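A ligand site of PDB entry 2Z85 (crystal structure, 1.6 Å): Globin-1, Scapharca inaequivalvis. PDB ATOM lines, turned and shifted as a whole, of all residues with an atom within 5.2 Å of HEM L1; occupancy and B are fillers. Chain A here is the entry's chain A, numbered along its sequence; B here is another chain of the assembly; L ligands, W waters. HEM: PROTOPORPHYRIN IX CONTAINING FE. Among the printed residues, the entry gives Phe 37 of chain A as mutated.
Tyr 50 touches HEM L1.
CZ of Phe 51 touches CHD of HEM L1, at 3.4 Å.
Leu 54 touches HEM L1.
His 69 touches HEM L1 (CE1 to CHA, 3.6 Å).
Thr 72 touches HEM L1.
Leu 73 touches HEM L1 (CG to C2B, 3.5 Å).
CB of Ala 76 touches CMB of HEM L1 (3.9 Å).
Leu 77 touches HEM L1.
Phe 97 touches HEM L1 (CE2 to CHB, 3.4 Å).
Ile 106 touches HEM L1.
Glu 110 touches HEM L1.
Phe 111 touches HEM L1.
Ile 114 touches HEM L1 (CG1 to CBB, 3.8 Å).
Hydrophobic or aromatic side chains that line HEM L1: Tyr 50, Phe 51, Leu 54, His 69, Leu 73, Ala 76, Leu 77, Phe 97, His 101, Ile 106, Phe 111 and Ile 114.
The nearest printed residue that does not touch HEM L1 is Thr 47 (4.05 Å).
Water W2 lies within hydrogen-bond range of O2A of HEM L1 (2.6 Å) and O of Phe 97 (3.1 Å).
Water W4 bridges an oxygen (O1A) of HEM L1 and the side-chain amino group (NZ) of Lys 96 of chain B.
A ring nitrogen (ND1) of His 101 is in hydrogen-bond range of the backbone carbonyl oxygen (O) of Phe 97.
O of His 101 is in hydrogen-bond range of N of Ile 106 (3.0 Å).
A ring nitrogen (ND1) of His 69 is in hydrogen-bond range of the side-chain amino group (NZ) of Lys 96 of chain B, 3.0 Å away.
The side-chain amide nitrogen (ND2) of Asn 100 of chain A lies close to the side-chain amide nitrogen (ND2) of Asn 100 of chain B (3.4 Å).
OH of Tyr 50 is in hydrogen-bond range of OE1 of Glu 110 (2.7 Å).
A ring nitrogen (NE2) of His 101 binds an iron atom (FE) of HEM L1, 2.1 Å away.
The guanidinium group (NH2) of Arg 104 lies within salt-bridge range of an oxygen (O1A) of HEM L1 (2.6 Å).
The side-chain amino group (NZ) of Lys 96 of chain B is in salt-bridge range of an oxygen (O2D) of HEM L1 (2.6 Å).
The guanidinium group (NH2) of Arg 53 is in salt-bridge range of an oxygen (O2D) of HEM L1 (2.8 Å).
The side-chain amide nitrogen (ND2) of Asn 100 of chain B sits at hydrogen-bond distance from an oxygen (O1A) of HEM L1 (2.8 Å).
The side-chain amide nitrogen (ND2) of Asn 100 of chain A is in hydrogen-bond range of an oxygen (O2A) of HEM L1 (3.2 Å).
O2A of HEM L2 lies within hydrogen-bond range of ND2 of Asn 100 of chain B.
An oxygen (O1A) of HEM L2 is in hydrogen-bond range of the side-chain amide nitrogen (ND2) of Asn 100 of chain A.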
ATOM      1  N   LEU A  36      -2.784  21.994   6.240  1.00  0.00           N
ATOM      2  CA  LEU A  36      -2.393  20.763   5.581  1.00  0.00           C
ATOM      3  C   LEU A  36      -2.422  19.555   6.528  1.00  0.00           C
ATOM      4  O   LEU A  36      -3.019  18.526   6.235  1.00  0.00           O
ATOM      5  CB  LEU A  36      -0.983  20.922   5.009  1.00  0.00           C
ATOM      6  CG  LEU A  36      -0.489  19.808   4.082  1.00  0.00           C
ATOM      7  CD1 LEU A  36      -1.381  19.762   2.850  1.00  0.00           C
ATOM      8  CD2 LEU A  36       0.950  20.058   3.675  1.00  0.00           C
ATOM      9  N   PHE A  37      -1.739  19.689   7.668  1.00  0.00           N
ATOM     10  CA  PHE A  37      -1.697  18.605   8.640  1.00  0.00           C
ATOM     11  C   PHE A  37      -2.999  18.311   9.400  1.00  0.00           C
ATOM     12  O   PHE A  37      -3.311  17.174   9.654  1.00  0.00           O
ATOM     13  CB  PHE A  37      -0.548  18.805   9.642  1.00  0.00           C
ATOM     14  CG  PHE A  37       0.507  17.745   9.534  1.00  0.00           C
ATOM     15  CD1 PHE A  37       1.147  17.513   8.333  1.00  0.00           C
ATOM     16  CD2 PHE A  37       0.816  16.952  10.633  1.00  0.00           C
ATOM     17  CE1 PHE A  37       2.093  16.501   8.213  1.00  0.00           C
ATOM     18  CE2 PHE A  37       1.757  15.938  10.529  1.00  0.00           C
ATOM     19  CZ  PHE A  37       2.403  15.708   9.312  1.00  0.00           C
ATOM     20  N   LEU A  40      -4.968  16.222   7.247  1.00  0.00           N
ATOM     21  CA  LEU A  40      -4.479  14.855   7.213  1.00  0.00           C
ATOM     22  C   LEU A  40      -5.114  14.044   8.329  1.00  0.00           C
ATOM     23  O   LEU A  40      -5.595  12.934   8.107  1.00  0.00           O
ATOM     24  CB  LEU A  40      -2.949  14.833   7.375  1.00  0.00           C
ATOM     25  CG  LEU A  40      -2.320  13.435   7.477  1.00  0.00           C
ATOM     26  CD1 LEU A  40      -2.491  12.672   6.173  1.00  0.00           C
ATOM     27  CD2 LEU A  40      -0.846  13.574   7.827  1.00  0.00           C
ATOM     28  N   THR A  47      -3.562   7.928  11.043  1.00  0.00           N
ATOM     29  CA  THR A  47      -2.200   8.452  11.081  1.00  0.00           C
ATOM     30  C   THR A  47      -1.864   9.202  12.373  1.00  0.00           C
ATOM     31  O   THR A  47      -0.708   9.486  12.637  1.00  0.00           O
ATOM     32  CB  THR A  47      -1.934   9.414   9.896  1.00  0.00           C
ATOM     33  OG1 THR A  47      -2.801  10.552   9.994  1.00  0.00           O
ATOM     34  CG2 THR A  47      -2.158   8.707   8.566  1.00  0.00           C
ATOM     35  N   TYR A  50       1.000   8.047  14.871  1.00  0.00           N
ATOM     36  CA  TYR A  50       2.407   8.342  14.652  1.00  0.00           C
ATOM     37  C   TYR A  50       2.850   9.632  15.334  1.00  0.00           C
ATOM     38  O   TYR A  50       4.047   9.875  15.475  1.00  0.00           O
ATOM     39  CB  TYR A  50       2.697   8.487  13.156  1.00  0.00           C
ATOM     40  CG  TYR A  50       2.566   7.211  12.346  1.00  0.00           C
ATOM     41  CD1 TYR A  50       3.480   6.177  12.488  1.00  0.00           C
ATOM     42  CD2 TYR A  50       1.534   7.067  11.421  1.00  0.00           C
ATOM     43  CE1 TYR A  50       3.378   5.019  11.719  1.00  0.00           C
ATOM     44  CE2 TYR A  50       1.425   5.913  10.645  1.00  0.00           C
ATOM     45  CZ  TYR A  50       2.347   4.895  10.804  1.00  0.00           C
ATOM     46  OH  TYR A  50       2.239   3.761  10.038  1.00  0.00           O
ATOM     47  N   PHE A  51       1.887  10.435  15.756  1.00  0.00           N
ATOM     48  CA  PHE A  51       2.183  11.720  16.386  1.00  0.00           C
ATOM     49  C   PHE A  51       1.828  11.850  17.860  1.00  0.00           C
ATOM     50  O   PHE A  51       1.398  12.914  18.307  1.00  0.00           O
ATOM     51  CB  PHE A  51       1.479  12.818  15.585  1.00  0.00           C
ATOM     52  CG  PHE A  51       1.896  12.860  14.141  1.00  0.00           C
ATOM     53  CD1 PHE A  51       3.020  13.568  13.746  1.00  0.00           C
ATOM     54  CD2 PHE A  51       1.166  12.165  13.191  1.00  0.00           C
ATOM     55  CE1 PHE A  51       3.418  13.585  12.415  1.00  0.00           C
ATOM     56  CE2 PHE A  51       1.546  12.166  11.851  1.00  0.00           C
ATOM     57  CZ  PHE A  51       2.677  12.871  11.463  1.00  0.00           C
ATOM     58  N   ARG A  53       3.648  12.230  20.354  1.00  0.00           N
ATOM     59  CA  ARG A  53       4.432  13.274  21.007  1.00  0.00           C
ATOM     60  C   ARG A  53       3.820  14.666  20.903  1.00  0.00           C
ATOM     61  O   ARG A  53       4.057  15.512  21.771  1.00  0.00           O
ATOM     62  CB  ARG A  53       5.856  13.324  20.421  1.00  0.00           C
ATOM     63  CG  ARG A  53       6.798  14.242  21.199  1.00  0.00           C
ATOM     64  CD  ARG A  53       8.096  14.479  20.453  1.00  0.00           C
ATOM     65  NE  ARG A  53       7.943  15.427  19.356  1.00  0.00           N
ATOM     66  CZ  ARG A  53       7.892  16.756  19.494  1.00  0.00           C
ATOM     67  NH1 ARG A  53       7.997  17.301  20.691  1.00  0.00           N
ATOM     68  NH2 ARG A  53       7.748  17.522  18.430  1.00  0.00           N
ATOM     69  N   LEU A  54       3.031  14.902  19.868  1.00  0.00           N
ATOM     70  CA  LEU A  54       2.401  16.199  19.657  1.00  0.00           C
ATOM     71  C   LEU A  54       1.272  16.527  20.632  1.00  0.00           C
ATOM     72  O   LEU A  54       0.912  17.690  20.799  1.00  0.00           O
ATOM     73  CB  LEU A  54       1.893  16.311  18.221  1.00  0.00           C
ATOM     74  CG  LEU A  54       2.880  16.837  17.171  1.00  0.00           C
ATOM     75  CD1 LEU A  54       4.248  16.182  17.340  1.00  0.00           C
ATOM     76  CD2 LEU A  54       2.331  16.582  15.776  1.00  0.00           C
ATOM     77  N   HIS A  69       5.674  21.745  14.325  1.00  0.00           N
ATOM     78  CA  HIS A  69       5.845  20.700  13.317  1.00  0.00           C
ATOM     79  C   HIS A  69       5.329  21.158  11.950  1.00  0.00           C
ATOM     80  O   HIS A  69       5.961  20.914  10.916  1.00  0.00           O
ATOM     81  CB  HIS A  69       5.096  19.441  13.739  1.00  0.00           C
ATOM     82  CG  HIS A  69       5.053  18.391  12.677  1.00  0.00           C
ATOM     83  ND1 HIS A  69       6.154  17.644  12.356  1.00  0.00           N
ATOM     84  CD2 HIS A  69       4.031  18.044  11.855  1.00  0.00           C
ATOM     85  CE1 HIS A  69       5.789  16.868  11.364  1.00  0.00           C
ATOM     86  NE2 HIS A  69       4.512  17.072  11.016  1.00  0.00           N
ATOM     87  N   THR A  72       7.602  23.767  10.307  1.00  0.00           N
ATOM     88  CA  THR A  72       8.811  23.073   9.887  1.00  0.00           C
ATOM     89  C   THR A  72       8.631  22.217   8.651  1.00  0.00           C
ATOM     90  O   THR A  72       9.522  22.134   7.803  1.00  0.00           O
ATOM     91  CB  THR A  72       9.359  22.222  11.043  1.00  0.00           C
ATOM     92  OG1 THR A  72       9.648  23.083  12.156  1.00  0.00           O
ATOM     93  CG2 THR A  72      10.639  21.504  10.624  1.00  0.00           C
ATOM     94  N   LEU A  73       7.479  21.574   8.534  1.00  0.00           N
ATOM     95  CA  LEU A  73       7.184  20.724   7.391  1.00  0.00           C
ATOM     96  C   LEU A  73       7.243  21.509   6.093  1.00  0.00           C
ATOM     97  O   LEU A  73       7.719  21.029   5.068  1.00  0.00           O
ATOM     98  CB  LEU A  73       5.804  20.101   7.563  1.00  0.00           C
ATOM     99  CG  LEU A  73       5.145  19.382   6.391  1.00  0.00           C
ATOM    100  CD1 LEU A  73       4.136  18.404   6.922  1.00  0.00           C
ATOM    101  CD2 LEU A  73       4.473  20.366   5.434  1.00  0.00           C
ATOM    102  N   ALA A  76      10.520  21.877   4.351  1.00  0.00           N
ATOM    103  CA  ALA A  76      11.018  20.719   3.633  1.00  0.00           C
ATOM    104  C   ALA A  76      10.517  20.874   2.200  1.00  0.00           C
ATOM    105  O   ALA A  76      11.233  20.621   1.233  1.00  0.00           O
ATOM    106  CB  ALA A  76      10.494  19.430   4.248  1.00  0.00           C
ATOM    107  N   LEU A  77       9.267  21.289   2.057  1.00  0.00           N
ATOM    108  CA  LEU A  77       8.682  21.503   0.738  1.00  0.00           C
ATOM    109  C   LEU A  77       9.426  22.635   0.028  1.00  0.00           C
ATOM    110  O   LEU A  77       9.673  22.567  -1.174  1.00  0.00           O
ATOM    111  CB  LEU A  77       7.190  21.807   0.850  1.00  0.00           C
ATOM    112  CG  LEU A  77       6.323  20.684   1.425  1.00  0.00           C
ATOM    113  CD1 LEU A  77       4.865  21.138   1.481  1.00  0.00           C
ATOM    114  CD2 LEU A  77       6.455  19.435   0.559  1.00  0.00           C
ATOM    115  N   PHE A  80      12.581  21.204  -1.416  1.00  0.00           N
ATOM    116  CA  PHE A  80      12.338  20.461  -2.653  1.00  0.00           C
ATOM    117  C   PHE A  80      12.125  21.388  -3.852  1.00  0.00           C
ATOM    118  O   PHE A  80      12.713  21.189  -4.911  1.00  0.00           O
ATOM    119  CB  PHE A  80      11.107  19.545  -2.523  1.00  0.00           C
ATOM    120  CG  PHE A  80      11.218  18.518  -1.421  1.00  0.00           C
ATOM    121  CD1 PHE A  80      12.449  18.095  -0.948  1.00  0.00           C
ATOM    122  CD2 PHE A  80      10.062  17.951  -0.884  1.00  0.00           C
ATOM    123  CE1 PHE A  80      12.536  17.124   0.063  1.00  0.00           C
ATOM    124  CE2 PHE A  80      10.130  16.981   0.116  1.00  0.00           C
ATOM    125  CZ  PHE A  80      11.376  16.570   0.584  1.00  0.00           C
ATOM    126  N   PHE A  97      15.885  13.486   3.449  1.00  0.00           N
ATOM    127  CA  PHE A  97      14.581  13.654   4.074  1.00  0.00           C
ATOM    128  C   PHE A  97      13.961  12.315   4.461  1.00  0.00           C
ATOM    129  O   PHE A  97      13.336  12.193   5.527  1.00  0.00           O
ATOM    130  CB  PHE A  97      13.664  14.402   3.098  1.00  0.00           C
ATOM    131  CG  PHE A  97      12.213  14.414   3.491  1.00  0.00           C
ATOM    132  CD1 PHE A  97      11.359  13.398   3.103  1.00  0.00           C
ATOM    133  CD2 PHE A  97      11.699  15.470   4.236  1.00  0.00           C
ATOM    134  CE1 PHE A  97      10.005  13.430   3.443  1.00  0.00           C
ATOM    135  CE2 PHE A  97      10.349  15.515   4.580  1.00  0.00           C
ATOM    136  CZ  PHE A  97       9.502  14.485   4.179  1.00  0.00           C
ATOM    137  N   ASN A 100      14.765   9.762   8.343  1.00  0.00           N
ATOM    138  CA  ASN A 100      13.968   9.696   9.562  1.00  0.00           C
ATOM    139  C   ASN A 100      12.589   9.079   9.349  1.00  0.00           C
ATOM    140  O   ASN A 100      12.056   8.445  10.258  1.00  0.00           O
ATOM    141  CB  ASN A 100      13.805  11.091  10.185  1.00  0.00           C
ATOM    142  CG  ASN A 100      15.096  11.637  10.763  1.00  0.00           C
ATOM    143  OD1 ASN A 100      16.022  10.880  11.060  1.00  0.00           O
ATOM    144  ND2 ASN A 100      15.159  12.945  10.951  1.00  0.00           N
ATOM    145  N   HIS A 101      12.026   9.257   8.159  1.00  0.00           N
ATOM    146  CA  HIS A 101      10.715   8.684   7.901  1.00  0.00           C
ATOM    147  C   HIS A 101      10.810   7.162   7.761  1.00  0.00           C
ATOM    148  O   HIS A 101       9.890   6.436   8.137  1.00  0.00           O
ATOM    149  CB  HIS A 101      10.075   9.326   6.662  1.00  0.00           C
ATOM    150  CG  HIS A 101       9.622  10.736   6.886  1.00  0.00           C
ATOM    151  ND1 HIS A 101      10.437  11.836   6.769  1.00  0.00           N
ATOM    152  CD2 HIS A 101       8.421  11.219   7.308  1.00  0.00           C
ATOM    153  CE1 HIS A 101       9.726  12.938   7.112  1.00  0.00           C
ATOM    154  NE2 HIS A 101       8.488  12.616   7.446  1.00  0.00           N
ATOM    155  N   ARG A 104      10.902   5.596  11.122  1.00  0.00           N
ATOM    156  CA  ARG A 104       9.592   5.598  11.771  1.00  0.00           C
ATOM    157  C   ARG A 104       8.658   4.596  11.121  1.00  0.00           C
ATOM    158  O   ARG A 104       7.489   4.488  11.489  1.00  0.00           O
ATOM    159  CB  ARG A 104       8.966   6.998  11.683  1.00  0.00           C
ATOM    160  CG  ARG A 104       9.762   8.058  12.404  1.00  0.00           C
ATOM    161  CD  ARG A 104       9.130   9.419  12.215  1.00  0.00           C
ATOM    162  NE  ARG A 104       9.843  10.457  12.950  1.00  0.00           N
ATOM    163  CZ  ARG A 104      10.454  11.482  12.371  1.00  0.00           C
ATOM    164  NH1 ARG A 104      10.438  11.611  11.053  1.00  0.00           N
ATOM    165  NH2 ARG A 104      11.087  12.374  13.117  1.00  0.00           N
ATOM    166  N   ILE A 106       7.444   4.619   8.075  1.00  0.00           N
ATOM    167  CA  ILE A 106       6.403   5.253   7.274  1.00  0.00           C
ATOM    168  C   ILE A 106       6.594   4.747   5.851  1.00  0.00           C
ATOM    169  O   ILE A 106       7.604   5.051   5.216  1.00  0.00           O
ATOM    170  CB  ILE A 106       6.554   6.799   7.273  1.00  0.00           C
ATOM    171  CG1 ILE A 106       6.560   7.327   8.707  1.00  0.00           C
ATOM    172  CG2 ILE A 106       5.415   7.426   6.478  1.00  0.00           C
ATOM    173  CD1 ILE A 106       5.318   6.994   9.509  1.00  0.00           C
ATOM    174  N   GLU A 110       1.684   4.994   3.080  1.00  0.00           N
ATOM    175  CA  GLU A 110       1.315   5.842   4.207  1.00  0.00           C
ATOM    176  C   GLU A 110       1.596   7.304   3.876  1.00  0.00           C
ATOM    177  O   GLU A 110       0.766   8.173   4.118  1.00  0.00           O
ATOM    178  CB  GLU A 110       2.121   5.428   5.450  1.00  0.00           C
ATOM    179  CG  GLU A 110       1.533   5.930   6.756  1.00  0.00           C
ATOM    180  CD  GLU A 110       0.478   4.990   7.317  1.00  0.00           C
ATOM    181  OE1 GLU A 110       0.843   3.878   7.741  1.00  0.00           O
ATOM    182  OE2 GLU A 110      -0.715   5.373   7.333  1.00  0.00           O
ATOM    183  N   PHE A 111       2.779   7.564   3.331  1.00  0.00           N
ATOM    184  CA  PHE A 111       3.176   8.916   2.975  1.00  0.00           C
ATOM    185  C   PHE A 111       2.262   9.513   1.901  1.00  0.00           C
ATOM    186  O   PHE A 111       1.964  10.696   1.920  1.00  0.00           O
ATOM    187  CB  PHE A 111       4.626   8.904   2.471  1.00  0.00           C
ATOM    188  CG  PHE A 111       5.252  10.274   2.415  1.00  0.00           C
ATOM    189  CD1 PHE A 111       5.843  10.826   3.550  1.00  0.00           C
ATOM    190  CD2 PHE A 111       5.252  11.002   1.230  1.00  0.00           C
ATOM    191  CE1 PHE A 111       6.413  12.088   3.507  1.00  0.00           C
ATOM    192  CE2 PHE A 111       5.829  12.270   1.184  1.00  0.00           C
ATOM    193  CZ  PHE A 111       6.409  12.803   2.318  1.00  0.00           C
ATOM    194  N   ILE A 114      -0.802  12.054   2.033  1.00  0.00           N
ATOM    195  CA  ILE A 114      -0.697  13.505   2.100  1.00  0.00           C
ATOM    196  C   ILE A 114      -1.252  14.158   0.828  1.00  0.00           C
ATOM    197  O   ILE A 114      -1.535  15.360   0.818  1.00  0.00           O
ATOM    198  CB  ILE A 114       0.779  13.944   2.306  1.00  0.00           C
ATOM    199  CG1 ILE A 114       0.825  15.398   2.796  1.00  0.00           C
ATOM    200  CG2 ILE A 114       1.569  13.817   1.016  1.00  0.00           C
ATOM    201  CD1 ILE A 114       0.162  15.596   4.150  1.00  0.00           C
ATOM    202  N   ILE A 118      -3.097  17.904   0.331  1.00  0.00           N
ATOM    203  CA  ILE A 118      -2.478  18.864  -0.581  1.00  0.00           C
ATOM    204  C   ILE A 118      -3.492  19.317  -1.625  1.00  0.00           C
ATOM    205  O   ILE A 118      -3.562  20.503  -1.951  1.00  0.00           O
ATOM    206  CB  ILE A 118      -1.239  18.253  -1.283  1.00  0.00           C
ATOM    207  CG1 ILE A 118      -0.099  18.082  -0.268  1.00  0.00           C
ATOM    208  CG2 ILE A 118      -0.794  19.153  -2.436  1.00  0.00           C
ATOM    209  CD1 ILE A 118       1.169  17.479  -0.838  1.00  0.00           C
ATOM    210  N   LYS B  96      10.994  22.123  18.358  1.00  0.00           N
ATOM    211  CA  LYS B  96      10.736  21.051  17.385  1.00  0.00           C
ATOM    212  C   LYS B  96      12.072  20.585  16.823  1.00  0.00           C
ATOM    213  O   LYS B  96      12.326  19.393  16.667  1.00  0.00           O
ATOM    214  CB  LYS B  96       9.829  21.567  16.262  1.00  0.00           C
ATOM    215  CG  LYS B  96       9.840  20.762  14.971  1.00  0.00           C
ATOM    216  CD  LYS B  96       9.244  19.369  15.130  1.00  0.00           C
ATOM    217  CE  LYS B  96       9.264  18.623  13.808  1.00  0.00           C
ATOM    218  NZ  LYS B  96       8.704  17.247  13.920  1.00  0.00           N
ATOM    219  N   ASN B 100      15.106  15.818  17.696  1.00  0.00           N
ATOM    220  CA  ASN B 100      16.024  14.814  17.159  1.00  0.00           C
ATOM    221  C   ASN B 100      17.457  14.984  17.642  1.00  0.00           C
ATOM    222  O   ASN B 100      18.198  14.007  17.759  1.00  0.00           O
ATOM    223  CB  ASN B 100      16.008  14.826  15.625  1.00  0.00           C
ATOM    224  CG  ASN B 100      14.685  14.353  15.044  1.00  0.00           C
ATOM    225  OD1 ASN B 100      13.912  13.660  15.709  1.00  0.00           O
ATOM    226  ND2 ASN B 100      14.432  14.714  13.791  1.00  0.00           N
HETATM  227  CHA HEM L   1       8.737  14.787  11.103  1.00  0.00           C
HETATM  228  CHB HEM L   1       8.102  16.849   6.778  1.00  0.00           C
HETATM  229  CHC HEM L   1       4.494  13.757   5.876  1.00  0.00           C
HETATM  230  CHD HEM L   1       5.415  11.418   9.990  1.00  0.00           C
HETATM  231  C1A HEM L   1       8.975  15.527   9.944  1.00  0.00           C
HETATM  232  C2A HEM L   1       9.943  16.625   9.843  1.00  0.00           C
HETATM  233  C3A HEM L   1       9.726  17.220   8.647  1.00  0.00           C
HETATM  234  C4A HEM L   1       8.647  16.495   8.012  1.00  0.00           C
HETATM  235  CMA HEM L   1      10.524  18.387   8.052  1.00  0.00           C
HETATM  236  CAA HEM L   1      11.039  17.017  10.824  1.00  0.00           C
HETATM  237  CBA HEM L   1      12.359  16.292  10.605  1.00  0.00           C
HETATM  238  CGA HEM L   1      12.272  14.814  10.925  1.00  0.00           C
HETATM  239  O1A HEM L   1      12.156  14.477  12.123  1.00  0.00           O
HETATM  240  O2A HEM L   1      12.301  13.988   9.997  1.00  0.00           O
HETATM  241  C1B HEM L   1       7.084  16.164   6.145  1.00  0.00           C
HETATM  242  C2B HEM L   1       6.520  16.554   4.862  1.00  0.00           C
HETATM  243  C3B HEM L   1       5.500  15.685   4.588  1.00  0.00           C
HETATM  244  C4B HEM L   1       5.441  14.779   5.737  1.00  0.00           C
HETATM  245  CMB HEM L   1       7.051  17.690   3.977  1.00  0.00           C
HETATM  246  CAB HEM L   1       4.672  15.590   3.459  1.00  0.00           C
HETATM  247  CBB HEM L   1       4.384  16.639   2.497  1.00  0.00           C
HETATM  248  C1C HEM L   1       4.488  12.819   6.883  1.00  0.00           C
HETATM  249  C2C HEM L   1       3.500  11.741   6.969  1.00  0.00           C
HETATM  250  C3C HEM L   1       3.779  11.035   8.097  1.00  0.00           C
HETATM  251  C4C HEM L   1       4.934  11.702   8.709  1.00  0.00           C
HETATM  252  CMC HEM L   1       2.356  11.500   5.968  1.00  0.00           C
HETATM  253  CAC HEM L   1       3.148   9.907   8.622  1.00  0.00           C
HETATM  254  CBC HEM L   1       1.823   9.412   8.348  1.00  0.00           C
HETATM  255  C1D HEM L   1       6.346  12.192  10.686  1.00  0.00           C
HETATM  256  C2D HEM L   1       6.590  12.094  12.116  1.00  0.00           C
HETATM  257  C3D HEM L   1       7.455  13.068  12.446  1.00  0.00           C
HETATM  258  C4D HEM L   1       7.787  13.769  11.205  1.00  0.00           C
HETATM  259  CMD HEM L   1       5.911  11.157  13.129  1.00  0.00           C
HETATM  260  CAD HEM L   1       7.904  13.408  13.855  1.00  0.00           C
HETATM  261  CBD HEM L   1       6.923  14.361  14.511  1.00  0.00           C
HETATM  262  CGD HEM L   1       7.375  14.827  15.875  1.00  0.00           C
HETATM  263  O1D HEM L   1       7.413  14.001  16.811  1.00  0.00           O
HETATM  264  O2D HEM L   1       7.694  16.028  16.026  1.00  0.00           O
HETATM  265  NA  HEM L   1       8.239  15.412   8.773  1.00  0.00           N
HETATM  266  NB  HEM L   1       6.471  15.022   6.648  1.00  0.00           N
HETATM  267  NC  HEM L   1       5.388  12.766   7.929  1.00  0.00           N
HETATM  268  ND  HEM L   1       7.050  13.258  10.125  1.00  0.00           N
HETATM  269 FE   HEM L   1       7.032  13.896   8.226  1.00  0.00          FE
HETATM  270  CHA HEM L   2      20.459  16.335  11.300  1.00  0.00           C
HETATM  271  CHB HEM L   2      20.325  21.170  11.272  1.00  0.00           C
HETATM  272  CHC HEM L   2      24.237  21.293  14.093  1.00  0.00           C
HETATM  273  CHD HEM L   2      24.232  16.456  14.353  1.00  0.00           C
HETATM  274  C1A HEM L   2      20.027  17.641  11.145  1.00  0.00           C
HETATM  275  C2A HEM L   2      18.874  18.029  10.342  1.00  0.00           C
HETATM  276  C3A HEM L   2      18.857  19.384  10.342  1.00  0.00           C
HETATM  277  C4A HEM L   2      19.983  19.831  11.121  1.00  0.00           C
HETATM  278  CMA HEM L   2      17.752  20.246   9.744  1.00  0.00           C
HETATM  279  CAA HEM L   2      17.810  17.141   9.690  1.00  0.00           C
HETATM  280  CBA HEM L   2      16.621  16.859  10.603  1.00  0.00           C
HETATM  281  CGA HEM L   2      16.993  15.996  11.795  1.00  0.00           C
HETATM  282  O1A HEM L   2      17.262  14.785  11.603  1.00  0.00           O
HETATM  283  O2A HEM L   2      17.023  16.522  12.929  1.00  0.00           O
HETATM  284  C1B HEM L   2      21.365  21.622  12.081  1.00  0.00           C
HETATM  285  C2B HEM L   2      21.742  23.031  12.187  1.00  0.00           C
HETATM  286  C3B HEM L   2      22.892  23.083  12.913  1.00  0.00           C
HETATM  287  C4B HEM L   2      23.156  21.686  13.318  1.00  0.00           C
HETATM  288  CMB HEM L   2      20.945  24.200  11.609  1.00  0.00           C
HETATM  289  CAB HEM L   2      23.726  24.184  13.212  1.00  0.00           C
HETATM  290  CBB HEM L   2      23.365  25.588  13.316  1.00  0.00           C
HETATM  291  C1C HEM L   2      24.504  19.990  14.491  1.00  0.00           C
HETATM  292  C2C HEM L   2      25.720  19.613  15.236  1.00  0.00           C
HETATM  293  C3C HEM L   2      25.719  18.249  15.314  1.00  0.00           C
HETATM  294  C4C HEM L   2      24.508  17.805  14.632  1.00  0.00           C
HETATM  295  CMC HEM L   2      26.759  20.600  15.781  1.00  0.00           C
HETATM  296  CAC HEM L   2      26.692  17.397  15.898  1.00  0.00           C
HETATM  297  CBC HEM L   2      28.034  17.750  16.274  1.00  0.00           C
HETATM  298  C1D HEM L   2      23.211  16.008  13.532  1.00  0.00           C
HETATM  299  C2D HEM L   2      23.106  14.627  13.074  1.00  0.00           C
HETATM  300  C3D HEM L   2      22.087  14.595  12.172  1.00  0.00           C
HETATM  301  C4D HEM L   2      21.557  15.966  12.102  1.00  0.00           C
HETATM  302  CMD HEM L   2      24.013  13.440  13.444  1.00  0.00           C
HETATM  303  CAD HEM L   2      21.713  13.402  11.307  1.00  0.00           C
HETATM  304  CBD HEM L   2      22.608  13.338  10.078  1.00  0.00           C
HETATM  305  CGD HEM L   2      22.230  12.225   9.122  1.00  0.00           C
HETATM  306  O1D HEM L   2      22.460  11.043   9.462  1.00  0.00           O
HETATM  307  O2D HEM L   2      21.693  12.525   8.047  1.00  0.00           O
HETATM  308  NA  HEM L   2      20.652  18.758  11.701  1.00  0.00           N
HETATM  309  NB  HEM L   2      22.197  20.805  12.822  1.00  0.00           N
HETATM  310  NC  HEM L   2      23.760  18.865  14.136  1.00  0.00           N
HETATM  311  ND  HEM L   2      22.280  16.836  12.903  1.00  0.00           N
HETATM  312 FE   HEM L   2      21.992  18.806  13.188  1.00  0.00          FE
HETATM  313  O   HOH W   1       9.305  12.228  17.428  1.00  0.00           O
HETATM  314  O   HOH W   2      13.340  14.440   7.700  1.00  0.00           O
HETATM  315  O   HOH W   3       7.945  19.116  10.614  1.00  0.00           O
HETATM  316  O   HOH W   4      11.083  15.825  14.203  1.00  0.00           O
